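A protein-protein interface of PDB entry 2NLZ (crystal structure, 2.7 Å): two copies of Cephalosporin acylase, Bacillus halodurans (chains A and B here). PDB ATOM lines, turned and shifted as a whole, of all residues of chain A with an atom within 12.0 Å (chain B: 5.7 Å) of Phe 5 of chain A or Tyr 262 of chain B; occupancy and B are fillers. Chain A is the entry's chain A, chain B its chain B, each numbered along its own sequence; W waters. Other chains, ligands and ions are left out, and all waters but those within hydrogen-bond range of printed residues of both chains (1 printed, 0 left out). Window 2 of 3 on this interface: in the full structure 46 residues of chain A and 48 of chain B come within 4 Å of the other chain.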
ATOM      1  N   VAL A   3     -18.241   3.219  15.886  1.00  0.00           N
ATOM      2  CA  VAL A   3     -17.135   2.834  16.745  1.00  0.00           C
ATOM      3  C   VAL A   3     -16.612   3.992  17.584  1.00  0.00           C
ATOM      4  O   VAL A   3     -15.940   4.880  17.092  1.00  0.00           O
ATOM      5  CB  VAL A   3     -16.033   2.098  15.960  1.00  0.00           C
ATOM      6  CG1 VAL A   3     -16.152   0.615  16.180  1.00  0.00           C
ATOM      7  CG2 VAL A   3     -16.153   2.380  14.495  1.00  0.00           C
ATOM      8  N   MET A   4     -16.982   3.984  18.859  1.00  0.00           N
ATOM      9  CA  MET A   4     -16.770   5.116  19.748  1.00  0.00           C
ATOM     10  C   MET A   4     -15.899   4.646  20.873  1.00  0.00           C
ATOM     11  O   MET A   4     -15.155   3.733  20.698  1.00  0.00           O
ATOM     12  CB  MET A   4     -18.087   5.617  20.316  1.00  0.00           C
ATOM     13  CG  MET A   4     -18.625   6.861  19.674  1.00  0.00           C
ATOM     14  SD  MET A   4     -17.852   8.357  20.249  1.00  0.00           S
ATOM     15  CE  MET A   4     -17.433   9.029  18.661  1.00  0.00           C
ATOM     16  N   PHE A   5     -15.984   5.261  22.030  1.00  0.00           N
ATOM     17  CA  PHE A   5     -15.078   4.869  23.065  1.00  0.00           C
ATOM     18  C   PHE A   5     -15.649   4.329  24.337  1.00  0.00           C
ATOM     19  O   PHE A   5     -15.179   4.643  25.400  1.00  0.00           O
ATOM     20  CB  PHE A   5     -14.043   5.941  23.350  1.00  0.00           C
ATOM     21  CG  PHE A   5     -14.608   7.234  23.828  1.00  0.00           C
ATOM     22  CD1 PHE A   5     -15.326   8.016  23.012  1.00  0.00           C
ATOM     23  CD2 PHE A   5     -14.373   7.670  25.087  1.00  0.00           C
ATOM     24  CE1 PHE A   5     -15.798   9.186  23.457  1.00  0.00           C
ATOM     25  CE2 PHE A   5     -14.851   8.806  25.507  1.00  0.00           C
ATOM     26  CZ  PHE A   5     -15.553   9.565  24.710  1.00  0.00           C
ATOM     27  N   ASP A   6     -16.684   3.504  24.216  1.00  0.00           N
ATOM     28  CA  ASP A   6     -17.087   2.614  25.300  1.00  0.00           C
ATOM     29  C   ASP A   6     -18.146   1.620  24.837  1.00  0.00           C
ATOM     30  O   ASP A   6     -18.960   1.925  23.964  1.00  0.00           O
ATOM     31  CB  ASP A   6     -17.607   3.421  26.491  1.00  0.00           C
ATOM     32  CG  ASP A   6     -18.060   4.813  26.098  1.00  0.00           C
ATOM     33  OD1 ASP A   6     -17.208   5.615  25.660  1.00  0.00           O
ATOM     34  OD2 ASP A   6     -19.267   5.106  26.225  1.00  0.00           O
ATOM     35  N   PRO A   7     -18.131   0.428  25.426  1.00  0.00           N
ATOM     36  CA  PRO A   7     -19.272  -0.491  25.343  1.00  0.00           C
ATOM     37  C   PRO A   7     -20.083  -0.667  26.647  1.00  0.00           C
ATOM     38  O   PRO A   7     -20.327   0.292  27.385  1.00  0.00           O
ATOM     39  CB  PRO A   7     -18.621  -1.831  24.913  1.00  0.00           C
ATOM     40  CG  PRO A   7     -17.108  -1.628  25.053  1.00  0.00           C
ATOM     41  CD  PRO A   7     -16.895  -0.300  25.755  1.00  0.00           C
ATOM     42  N   GLN A   8     -20.503  -1.908  26.880  1.00  0.00           N
ATOM     43  CA  GLN A   8     -21.301  -2.319  28.029  1.00  0.00           C
ATOM     44  C   GLN A   8     -20.411  -3.282  28.850  1.00  0.00           C
ATOM     45  O   GLN A   8     -20.881  -4.219  29.515  1.00  0.00           O
ATOM     46  CB  GLN A   8     -22.542  -3.030  27.499  1.00  0.00           C
ATOM     47  CG  GLN A   8     -23.744  -3.095  28.422  1.00  0.00           C
ATOM     48  CD  GLN A   8     -24.932  -3.803  27.769  1.00  0.00           C
ATOM     49  OE1 GLN A   8     -25.076  -3.800  26.542  1.00  0.00           O
ATOM     50  NE2 GLN A   8     -25.785  -4.414  28.588  1.00  0.00           N
ATOM     51  N   SER A   9     -19.108  -3.023  28.787  1.00  0.00           N
ATOM     52  CA  SER A   9     -18.092  -3.873  29.388  1.00  0.00           C
ATOM     53  C   SER A   9     -17.669  -3.374  30.770  1.00  0.00           C
ATOM     54  O   SER A   9     -17.394  -2.190  30.958  1.00  0.00           O
ATOM     55  CB  SER A   9     -16.878  -3.944  28.456  1.00  0.00           C
ATOM     56  OG  SER A   9     -15.692  -4.268  29.164  1.00  0.00           O
ATOM     57  N   TYR A  10     -17.612  -4.291  31.730  1.00  0.00           N
ATOM     58  CA  TYR A  10     -17.201  -3.956  33.087  1.00  0.00           C
ATOM     59  C   TYR A  10     -16.139  -4.933  33.552  1.00  0.00           C
ATOM     60  O   TYR A  10     -16.450  -5.902  34.251  1.00  0.00           O
ATOM     61  CB  TYR A  10     -18.405  -3.989  34.031  1.00  0.00           C
ATOM     62  CG  TYR A  10     -19.462  -2.955  33.707  1.00  0.00           C
ATOM     63  CD1 TYR A  10     -19.362  -1.654  34.191  1.00  0.00           C
ATOM     64  CD2 TYR A  10     -20.561  -3.279  32.919  1.00  0.00           C
ATOM     65  CE1 TYR A  10     -20.329  -0.704  33.899  1.00  0.00           C
ATOM     66  CE2 TYR A  10     -21.528  -2.335  32.624  1.00  0.00           C
ATOM     67  CZ  TYR A  10     -21.403  -1.045  33.115  1.00  0.00           C
ATOM     68  OH  TYR A  10     -22.362  -0.096  32.833  1.00  0.00           O
ATOM     69  N   PRO A  11     -14.876  -4.693  33.158  1.00  0.00           N
ATOM     70  CA  PRO A  11     -13.806  -5.660  33.426  1.00  0.00           C
ATOM     71  C   PRO A  11     -13.424  -5.765  34.904  1.00  0.00           C
ATOM     72  O   PRO A  11     -12.833  -6.767  35.314  1.00  0.00           O
ATOM     73  CB  PRO A  11     -12.616  -5.124  32.605  1.00  0.00           C
ATOM     74  CG  PRO A  11     -13.167  -4.041  31.734  1.00  0.00           C
ATOM     75  CD  PRO A  11     -14.378  -3.513  32.434  1.00  0.00           C
ATOM     76  N   TYR A  12     -13.763  -4.747  35.692  1.00  0.00           N
ATOM     77  CA  TYR A  12     -13.279  -4.647  37.074  1.00  0.00           C
ATOM     78  C   TYR A  12     -14.431  -4.660  38.061  1.00  0.00           C
ATOM     79  O   TYR A  12     -15.538  -4.255  37.724  1.00  0.00           O
ATOM     80  CB  TYR A  12     -12.385  -3.398  37.249  1.00  0.00           C
ATOM     81  CG  TYR A  12     -11.370  -3.246  36.135  1.00  0.00           C
ATOM     82  CD1 TYR A  12     -10.271  -4.101  36.048  1.00  0.00           C
ATOM     83  CD2 TYR A  12     -11.532  -2.277  35.146  1.00  0.00           C
ATOM     84  CE1 TYR A  12      -9.349  -3.982  35.018  1.00  0.00           C
ATOM     85  CE2 TYR A  12     -10.622  -2.153  34.112  1.00  0.00           C
ATOM     86  CZ  TYR A  12      -9.533  -3.008  34.053  1.00  0.00           C
ATOM     87  OH  TYR A  12      -8.628  -2.890  33.032  1.00  0.00           O
ATOM     88  N   ILE B 257      -3.022  19.091  25.231  1.00  0.00           N
ATOM     89  CA  ILE B 257      -2.126  18.170  24.558  1.00  0.00           C
ATOM     90  C   ILE B 257      -3.006  17.347  23.619  1.00  0.00           C
ATOM     91  O   ILE B 257      -4.108  16.953  23.994  1.00  0.00           O
ATOM     92  CB  ILE B 257      -1.397  17.266  25.602  1.00  0.00           C
ATOM     93  CG1 ILE B 257      -0.103  17.930  26.058  1.00  0.00           C
ATOM     94  CG2 ILE B 257      -1.111  15.851  25.077  1.00  0.00           C
ATOM     95  CD1 ILE B 257       0.804  18.368  24.918  1.00  0.00           C
ATOM     96  N   ASP B 258      -2.556  17.126  22.389  1.00  0.00           N
ATOM     97  CA  ASP B 258      -3.222  16.157  21.542  1.00  0.00           C
ATOM     98  C   ASP B 258      -2.804  14.785  22.041  1.00  0.00           C
ATOM     99  O   ASP B 258      -1.632  14.430  21.961  1.00  0.00           O
ATOM    100  CB  ASP B 258      -2.835  16.338  20.073  1.00  0.00           C
ATOM    101  CG  ASP B 258      -3.710  15.521  19.130  1.00  0.00           C
ATOM    102  OD1 ASP B 258      -3.525  14.294  19.028  1.00  0.00           O
ATOM    103  OD2 ASP B 258      -4.581  16.117  18.473  1.00  0.00           O
ATOM    104  N   TYR B 259      -3.747  14.036  22.601  1.00  0.00           N
ATOM    105  CA  TYR B 259      -3.481  12.649  22.969  1.00  0.00           C
ATOM    106  C   TYR B 259      -4.321  11.699  22.120  1.00  0.00           C
ATOM    107  O   TYR B 259      -5.485  11.454  22.417  1.00  0.00           O
ATOM    108  CB  TYR B 259      -3.688  12.406  24.465  1.00  0.00           C
ATOM    109  CG  TYR B 259      -3.175  11.057  24.935  1.00  0.00           C
ATOM    110  CD1 TYR B 259      -1.828  10.863  25.230  1.00  0.00           C
ATOM    111  CD2 TYR B 259      -4.039   9.975  25.084  1.00  0.00           C
ATOM    112  CE1 TYR B 259      -1.359   9.635  25.660  1.00  0.00           C
ATOM    113  CE2 TYR B 259      -3.577   8.745  25.512  1.00  0.00           C
ATOM    114  CZ  TYR B 259      -2.239   8.576  25.797  1.00  0.00           C
ATOM    115  OH  TYR B 259      -1.789   7.338  26.212  1.00  0.00           O
ATOM    116  N   ARG B 260      -3.699  11.185  21.056  1.00  0.00           N
ATOM    117  CA  ARG B 260      -4.283  10.205  20.133  1.00  0.00           C
ATOM    118  C   ARG B 260      -5.579  10.666  19.515  1.00  0.00           C
ATOM    119  O   ARG B 260      -6.528   9.891  19.407  1.00  0.00           O
ATOM    120  CB  ARG B 260      -4.454   8.850  20.819  1.00  0.00           C
ATOM    121  CG  ARG B 260      -3.301   8.560  21.741  1.00  0.00           C
ATOM    122  CD  ARG B 260      -3.055   7.114  21.930  1.00  0.00           C
ATOM    123  NE  ARG B 260      -2.012   6.925  22.928  1.00  0.00           N
ATOM    124  CZ  ARG B 260      -0.729   6.752  22.644  1.00  0.00           C
ATOM    125  NH1 ARG B 260      -0.325   6.728  21.386  1.00  0.00           N
ATOM    126  NH2 ARG B 260       0.149   6.586  23.622  1.00  0.00           N
ATOM    127  N   GLY B 261      -5.596  11.936  19.112  1.00  0.00           N
ATOM    128  CA  GLY B 261      -6.745  12.556  18.455  1.00  0.00           C
ATOM    129  C   GLY B 261      -7.527  13.463  19.386  1.00  0.00           C
ATOM    130  O   GLY B 261      -8.076  14.485  18.964  1.00  0.00           O
ATOM    131  N   TYR B 262      -7.579  13.075  20.657  1.00  0.00           N
ATOM    132  CA  TYR B 262      -8.335  13.810  21.660  1.00  0.00           C
ATOM    133  C   TYR B 262      -7.462  14.940  22.162  1.00  0.00           C
ATOM    134  O   TYR B 262      -6.262  14.935  21.925  1.00  0.00           O
ATOM    135  CB  TYR B 262      -8.728  12.897  22.832  1.00  0.00           C
ATOM    136  CG  TYR B 262      -9.749  11.821  22.516  1.00  0.00           C
ATOM    137  CD1 TYR B 262     -11.065  11.939  22.945  1.00  0.00           C
ATOM    138  CD2 TYR B 262      -9.397  10.676  21.809  1.00  0.00           C
ATOM    139  CE1 TYR B 262     -12.013  10.955  22.668  1.00  0.00           C
ATOM    140  CE2 TYR B 262     -10.333   9.686  21.526  1.00  0.00           C
ATOM    141  CZ  TYR B 262     -11.640   9.834  21.961  1.00  0.00           C
ATOM    142  OH  TYR B 262     -12.567   8.861  21.676  1.00  0.00           O
ATOM    143  N   ARG B 263      -8.065  15.913  22.838  1.00  0.00           N
ATOM    144  CA  ARG B 263      -7.304  16.943  23.531  1.00  0.00           C
ATOM    145  C   ARG B 263      -7.640  16.943  25.010  1.00  0.00           C
ATOM    146  O   ARG B 263      -8.804  17.068  25.410  1.00  0.00           O
ATOM    147  CB  ARG B 263      -7.503  18.327  22.911  1.00  0.00           C
ATOM    148  CG  ARG B 263      -6.936  18.456  21.500  1.00  0.00           C
ATOM    149  CD  ARG B 263      -6.609  19.894  21.147  1.00  0.00           C
ATOM    150  NE  ARG B 263      -5.308  20.298  21.664  1.00  0.00           N
ATOM    151  CZ  ARG B 263      -4.154  20.120  21.025  1.00  0.00           C
ATOM    152  NH1 ARG B 263      -4.127  19.538  19.830  1.00  0.00           N
ATOM    153  NH2 ARG B 263      -3.022  20.530  21.583  1.00  0.00           N
ATOM    154  N   VAL B 264      -6.602  16.780  25.820  1.00  0.00           N
ATOM    155  CA  VAL B 264      -6.747  16.707  27.257  1.00  0.00           C
ATOM    156  C   VAL B 264      -6.457  18.087  27.819  1.00  0.00           C
ATOM    157  O   VAL B 264      -5.379  18.618  27.604  1.00  0.00           O
ATOM    158  CB  VAL B 264      -5.775  15.671  27.851  1.00  0.00           C
ATOM    159  CG1 VAL B 264      -5.953  15.577  29.358  1.00  0.00           C
ATOM    160  CG2 VAL B 264      -5.990  14.307  27.209  1.00  0.00           C
ATOM    161  N   LEU B 426     -12.088  16.926  28.666  1.00  0.00           N
ATOM    162  CA  LEU B 426     -11.748  16.164  27.461  1.00  0.00           C
ATOM    163  C   LEU B 426     -12.519  16.642  26.229  1.00  0.00           C
ATOM    164  O   LEU B 426     -13.731  16.833  26.276  1.00  0.00           O
ATOM    165  CB  LEU B 426     -11.967  14.660  27.684  1.00  0.00           C
ATOM    166  CG  LEU B 426     -11.361  13.727  26.621  1.00  0.00           C
ATOM    167  CD1 LEU B 426      -9.900  14.054  26.308  1.00  0.00           C
ATOM    168  CD2 LEU B 426     -11.492  12.280  27.058  1.00  0.00           C
ATOM    169  N   THR B 427     -11.792  16.792  25.128  1.00  0.00           N
ATOM    170  CA  THR B 427     -12.307  17.353  23.881  1.00  0.00           C
ATOM    171  C   THR B 427     -11.823  16.523  22.687  1.00  0.00           C
ATOM    172  O   THR B 427     -10.718  15.997  22.715  1.00  0.00           O
ATOM    173  CB  THR B 427     -11.816  18.815  23.762  1.00  0.00           C
ATOM    174  OG1 THR B 427     -12.687  19.680  24.508  1.00  0.00           O
ATOM    175  CG2 THR B 427     -11.768  19.289  22.346  1.00  0.00           C
ATOM    176  N   LYS B 428     -12.647  16.379  21.652  1.00  0.00           N
ATOM    177  CA  LYS B 428     -12.208  15.733  20.411  1.00  0.00           C
ATOM    178  C   LYS B 428     -12.717  16.494  19.190  1.00  0.00           C
ATOM    179  O   LYS B 428     -13.924  16.607  18.986  1.00  0.00           O
ATOM    180  CB  LYS B 428     -12.661  14.268  20.362  1.00  0.00           C
ATOM    181  CG  LYS B 428     -12.197  13.479  19.137  1.00  0.00           C
ATOM    182  CD  LYS B 428     -12.856  12.093  19.080  1.00  0.00           C
ATOM    183  CE  LYS B 428     -12.524  11.336  17.792  1.00  0.00           C
ATOM    184  NZ  LYS B 428     -11.066  11.026  17.680  1.00  0.00           N
ATOM    185  N   ILE B 433     -16.293  16.602  24.951  1.00  0.00           N
ATOM    186  CA  ILE B 433     -16.758  15.300  25.390  1.00  0.00           C
ATOM    187  C   ILE B 433     -16.949  15.201  26.902  1.00  0.00           C
ATOM    188  O   ILE B 433     -17.816  14.466  27.360  1.00  0.00           O
ATOM    189  CB  ILE B 433     -16.002  14.089  24.767  1.00  0.00           C
ATOM    190  CG1 ILE B 433     -14.786  13.721  25.578  1.00  0.00           C
ATOM    191  CG2 ILE B 433     -15.659  14.311  23.284  1.00  0.00           C
ATOM    192  CD1 ILE B 433     -14.368  12.312  25.312  1.00  0.00           C
ATOM    193  N   THR B 455      -9.638   5.754  29.221  1.00  0.00           N
ATOM    194  CA  THR B 455     -10.702   6.161  28.311  1.00  0.00           C
ATOM    195  C   THR B 455     -10.257   6.123  26.850  1.00  0.00           C
ATOM    196  O   THR B 455     -10.886   5.468  26.016  1.00  0.00           O
ATOM    197  CB  THR B 455     -11.225   7.572  28.646  1.00  0.00           C
ATOM    198  OG1 THR B 455     -11.599   7.633  30.028  1.00  0.00           O
ATOM    199  CG2 THR B 455     -12.427   7.904  27.792  1.00  0.00           C
ATOM    200  N   ILE B 456      -9.166   6.822  26.549  1.00  0.00           N
ATOM    201  CA  ILE B 456      -8.717   7.008  25.164  1.00  0.00           C
ATOM    202  C   ILE B 456      -7.998   5.772  24.610  1.00  0.00           C
ATOM    203  O   ILE B 456      -8.323   5.292  23.518  1.00  0.00           O
ATOM    204  CB  ILE B 456      -7.831   8.251  25.058  1.00  0.00           C
ATOM    205  CG1 ILE B 456      -8.648   9.499  25.429  1.00  0.00           C
ATOM    206  CG2 ILE B 456      -7.254   8.379  23.678  1.00  0.00           C
ATOM    207  CD1 ILE B 456      -7.805  10.673  25.928  1.00  0.00           C
ATOM    208  N   GLY B 459     -10.520   2.166  26.143  1.00  0.00           N
ATOM    209  CA  GLY B 459     -11.945   2.109  25.808  1.00  0.00           C
ATOM    210  C   GLY B 459     -12.899   1.765  26.939  1.00  0.00           C
ATOM    211  O   GLY B 459     -13.964   1.194  26.701  1.00  0.00           O
ATOM    212  N   LEU B 460     -12.519   2.118  28.165  1.00  0.00           N
ATOM    213  CA  LEU B 460     -13.347   1.872  29.337  1.00  0.00           C
ATOM    214  C   LEU B 460     -14.445   2.908  29.420  1.00  0.00           C
ATOM    215  O   LEU B 460     -14.221   4.072  29.099  1.00  0.00           O
ATOM    216  CB  LEU B 460     -12.495   1.899  30.609  1.00  0.00           C
ATOM    217  CG  LEU B 460     -11.894   0.576  31.102  1.00  0.00           C
ATOM    218  CD1 LEU B 460     -11.853  -0.518  30.045  1.00  0.00           C
ATOM    219  CD2 LEU B 460     -10.512   0.827  31.630  1.00  0.00           C
ATOM    220  N   ASN B 461     -15.631   2.484  29.838  1.00  0.00           N
ATOM    221  CA  ASN B 461     -16.713   3.433  30.092  1.00  0.00           C
ATOM    222  C   ASN B 461     -16.420   4.285  31.335  1.00  0.00           C
ATOM    223  O   ASN B 461     -15.533   3.940  32.120  1.00  0.00           O
ATOM    224  CB  ASN B 461     -18.079   2.727  30.158  1.00  0.00           C
ATOM    225  CG  ASN B 461     -18.240   1.856  31.376  1.00  0.00           C
ATOM    226  OD1 ASN B 461     -18.007   2.277  32.509  1.00  0.00           O
ATOM    227  ND2 ASN B 461     -18.689   0.637  31.152  1.00  0.00           N
ATOM    228  N   TRP B 516     -19.302  11.856  30.299  1.00  0.00           N
ATOM    229  CA  TRP B 516     -18.987  11.997  28.876  1.00  0.00           C
ATOM    230  C   TRP B 516     -20.246  12.309  28.077  1.00  0.00           C
ATOM    231  O   TRP B 516     -21.319  11.780  28.351  1.00  0.00           O
ATOM    232  CB  TRP B 516     -18.282  10.775  28.261  1.00  0.00           C
ATOM    233  CG  TRP B 516     -16.933  10.350  28.836  1.00  0.00           C
ATOM    234  CD1 TRP B 516     -16.489   9.059  28.982  1.00  0.00           C
ATOM    235  CD2 TRP B 516     -15.863  11.194  29.317  1.00  0.00           C
ATOM    236  NE1 TRP B 516     -15.224   9.049  29.526  1.00  0.00           N
ATOM    237  CE2 TRP B 516     -14.815  10.340  29.737  1.00  0.00           C
ATOM    238  CE3 TRP B 516     -15.697  12.577  29.452  1.00  0.00           C
ATOM    239  CZ2 TRP B 516     -13.624  10.822  30.277  1.00  0.00           C
ATOM    240  CZ3 TRP B 516     -14.500  13.054  29.989  1.00  0.00           C
ATOM    241  CH2 TRP B 516     -13.486  12.176  30.394  1.00  0.00           C
ATOM    242  N   ARG B 517     -20.096  13.177  27.082  1.00  0.00           N
ATOM    243  CA  ARG B 517     -21.179  13.505  26.175  1.00  0.00           C
ATOM    244  C   ARG B 517     -20.838  12.978  24.789  1.00  0.00           C
ATOM    245  O   ARG B 517     -19.750  13.217  24.273  1.00  0.00           O
ATOM    246  CB  ARG B 517     -21.385  15.019  26.141  1.00  0.00           C
ATOM    247  CG  ARG B 517     -22.379  15.501  25.113  1.00  0.00           C
ATOM    248  CD  ARG B 517     -22.196  16.976  24.849  1.00  0.00           C
ATOM    249  NE  ARG B 517     -22.854  17.364  23.614  1.00  0.00           N
ATOM    250  CZ  ARG B 517     -24.076  17.875  23.533  1.00  0.00           C
ATOM    251  NH1 ARG B 517     -24.801  18.094  24.625  1.00  0.00           N
ATOM    252  NH2 ARG B 517     -24.570  18.174  22.343  1.00  0.00           N
HETATM  253  O   HOH W   1     -16.019  -0.192  29.102  1.00  0.00           O
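Among the printed residues, pairs that only touch across the chains: Phe 5 of chain A with Ile 433 of chain B, Phe 5 of chain A with Tyr 262 of chain B, Phe 5 of chain A with Thr 455 of chain B, Pro 7 of chain A with Gly 459 of chain B, Tyr 10 of chain A with Asn 461 of chain B, Asp 6 of chain A with Gly 459 of chain B, Asp 6 of chain A with Asn 461 of chain B, Phe 5 of chain A with Trp 516 of chain B, Phe 5 of chain A with Leu 460 of chain B, Tyr 12 of chain A with Leu 460 of chain B and Phe 5 of chain A with Gly 459 of chain B.
Of the 10 printed residues of chain A, 6 touch a printed residue of chain B. Printed residues of chain A that touch a printed residue of chain B: Phe 5, Asp 6, Pro 7, Ser 9, Tyr 10 and Tyr 12. Hydrophobic or aromatic side chains of chain A that line the printed part of chain B: Phe 5, Pro 7, Tyr 10 and Tyr 12. Among the printed residues, no Asp or Glu carboxylate lies within 4 Å of a Lys or Arg side-chain nitrogen of the other chain.
O of Ser 9 of chain A is in hydrogen-bond range of ND2 of Asn 461 of chain B (3.1 Å).
The backbone NH (N) of Ile 433 of chain B lies within hydrogen-bond range of the backbone carbonyl oxygen (O) of Leu 426 of chain B (2.9 Å). The backbone carbonyl oxygen (O) of Ile 433 of chain B sits at hydrogen-bond distance from the backbone NH (N) of Arg 517 of chain B.
No position is printed for both chains. Of the 12 pairs that touch across the chains among the printed residues, none has its exchanged pair printed and touching as well.
Water W1 lies within hydrogen-bond range of N of Asn 461 of chain B (2.8 Å), O of Ser 9 of chain A (3.1 Å) and O of Gly 459 of chain B (3.5 Å).
Val 3 of chain A touches none of the printed residues of chain B. Of chain B, only Tyr 262, Ile 433, Thr 455, Gly 459, Leu 460 and Trp 516 come within 4 Å of Phe 5 of chain A. Of the printed residues of chain B, Pro 7 of chain A touches Gly 459 (3.4 Å). No residue of chain A comes within 4 Å of Asp 258 of chain B. No residue of chain A comes within 4 Å of Gly 261 of chain B. No residue of chain A comes within 4 Å of Arg 263 of chain B. Lys 428 of chain B touches none of the printed residues of chain A. Ile 433 of chain B touches just one residue of chain A: Phe 5 (3.1 Å). Of chain A, only Phe 5 (3.3 Å) comes within 4 Å of Thr 455 of chain B. Ile 456 of chain B touches none of the printed residues of chain A. Of the printed residues of chain A, Gly 459 of chain B touches Phe 5, Asp 6 and Pro 7. Printed residues of chain A within 4 Å of Leu 460 of chain B: Phe 5 (3.9 Å) and Tyr 12 (3.9 Å). Printed residues of chain A within 4 Å of Asn 461 of chain B: Asp 6 (3.7 Å), Ser 9 (3.1 Å) and Tyr 10 (3.5 Å). Arg 517 of chain B touches none of the printed residues of chain A. The nearest residue of chain A that does not touch Tyr 262 of chain B is Met 4 of chain A (5.4 Å). The nearest printed residue of chain B that does not touch Ser 9 of chain A is Leu 460 of chain B (5.4 Å).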
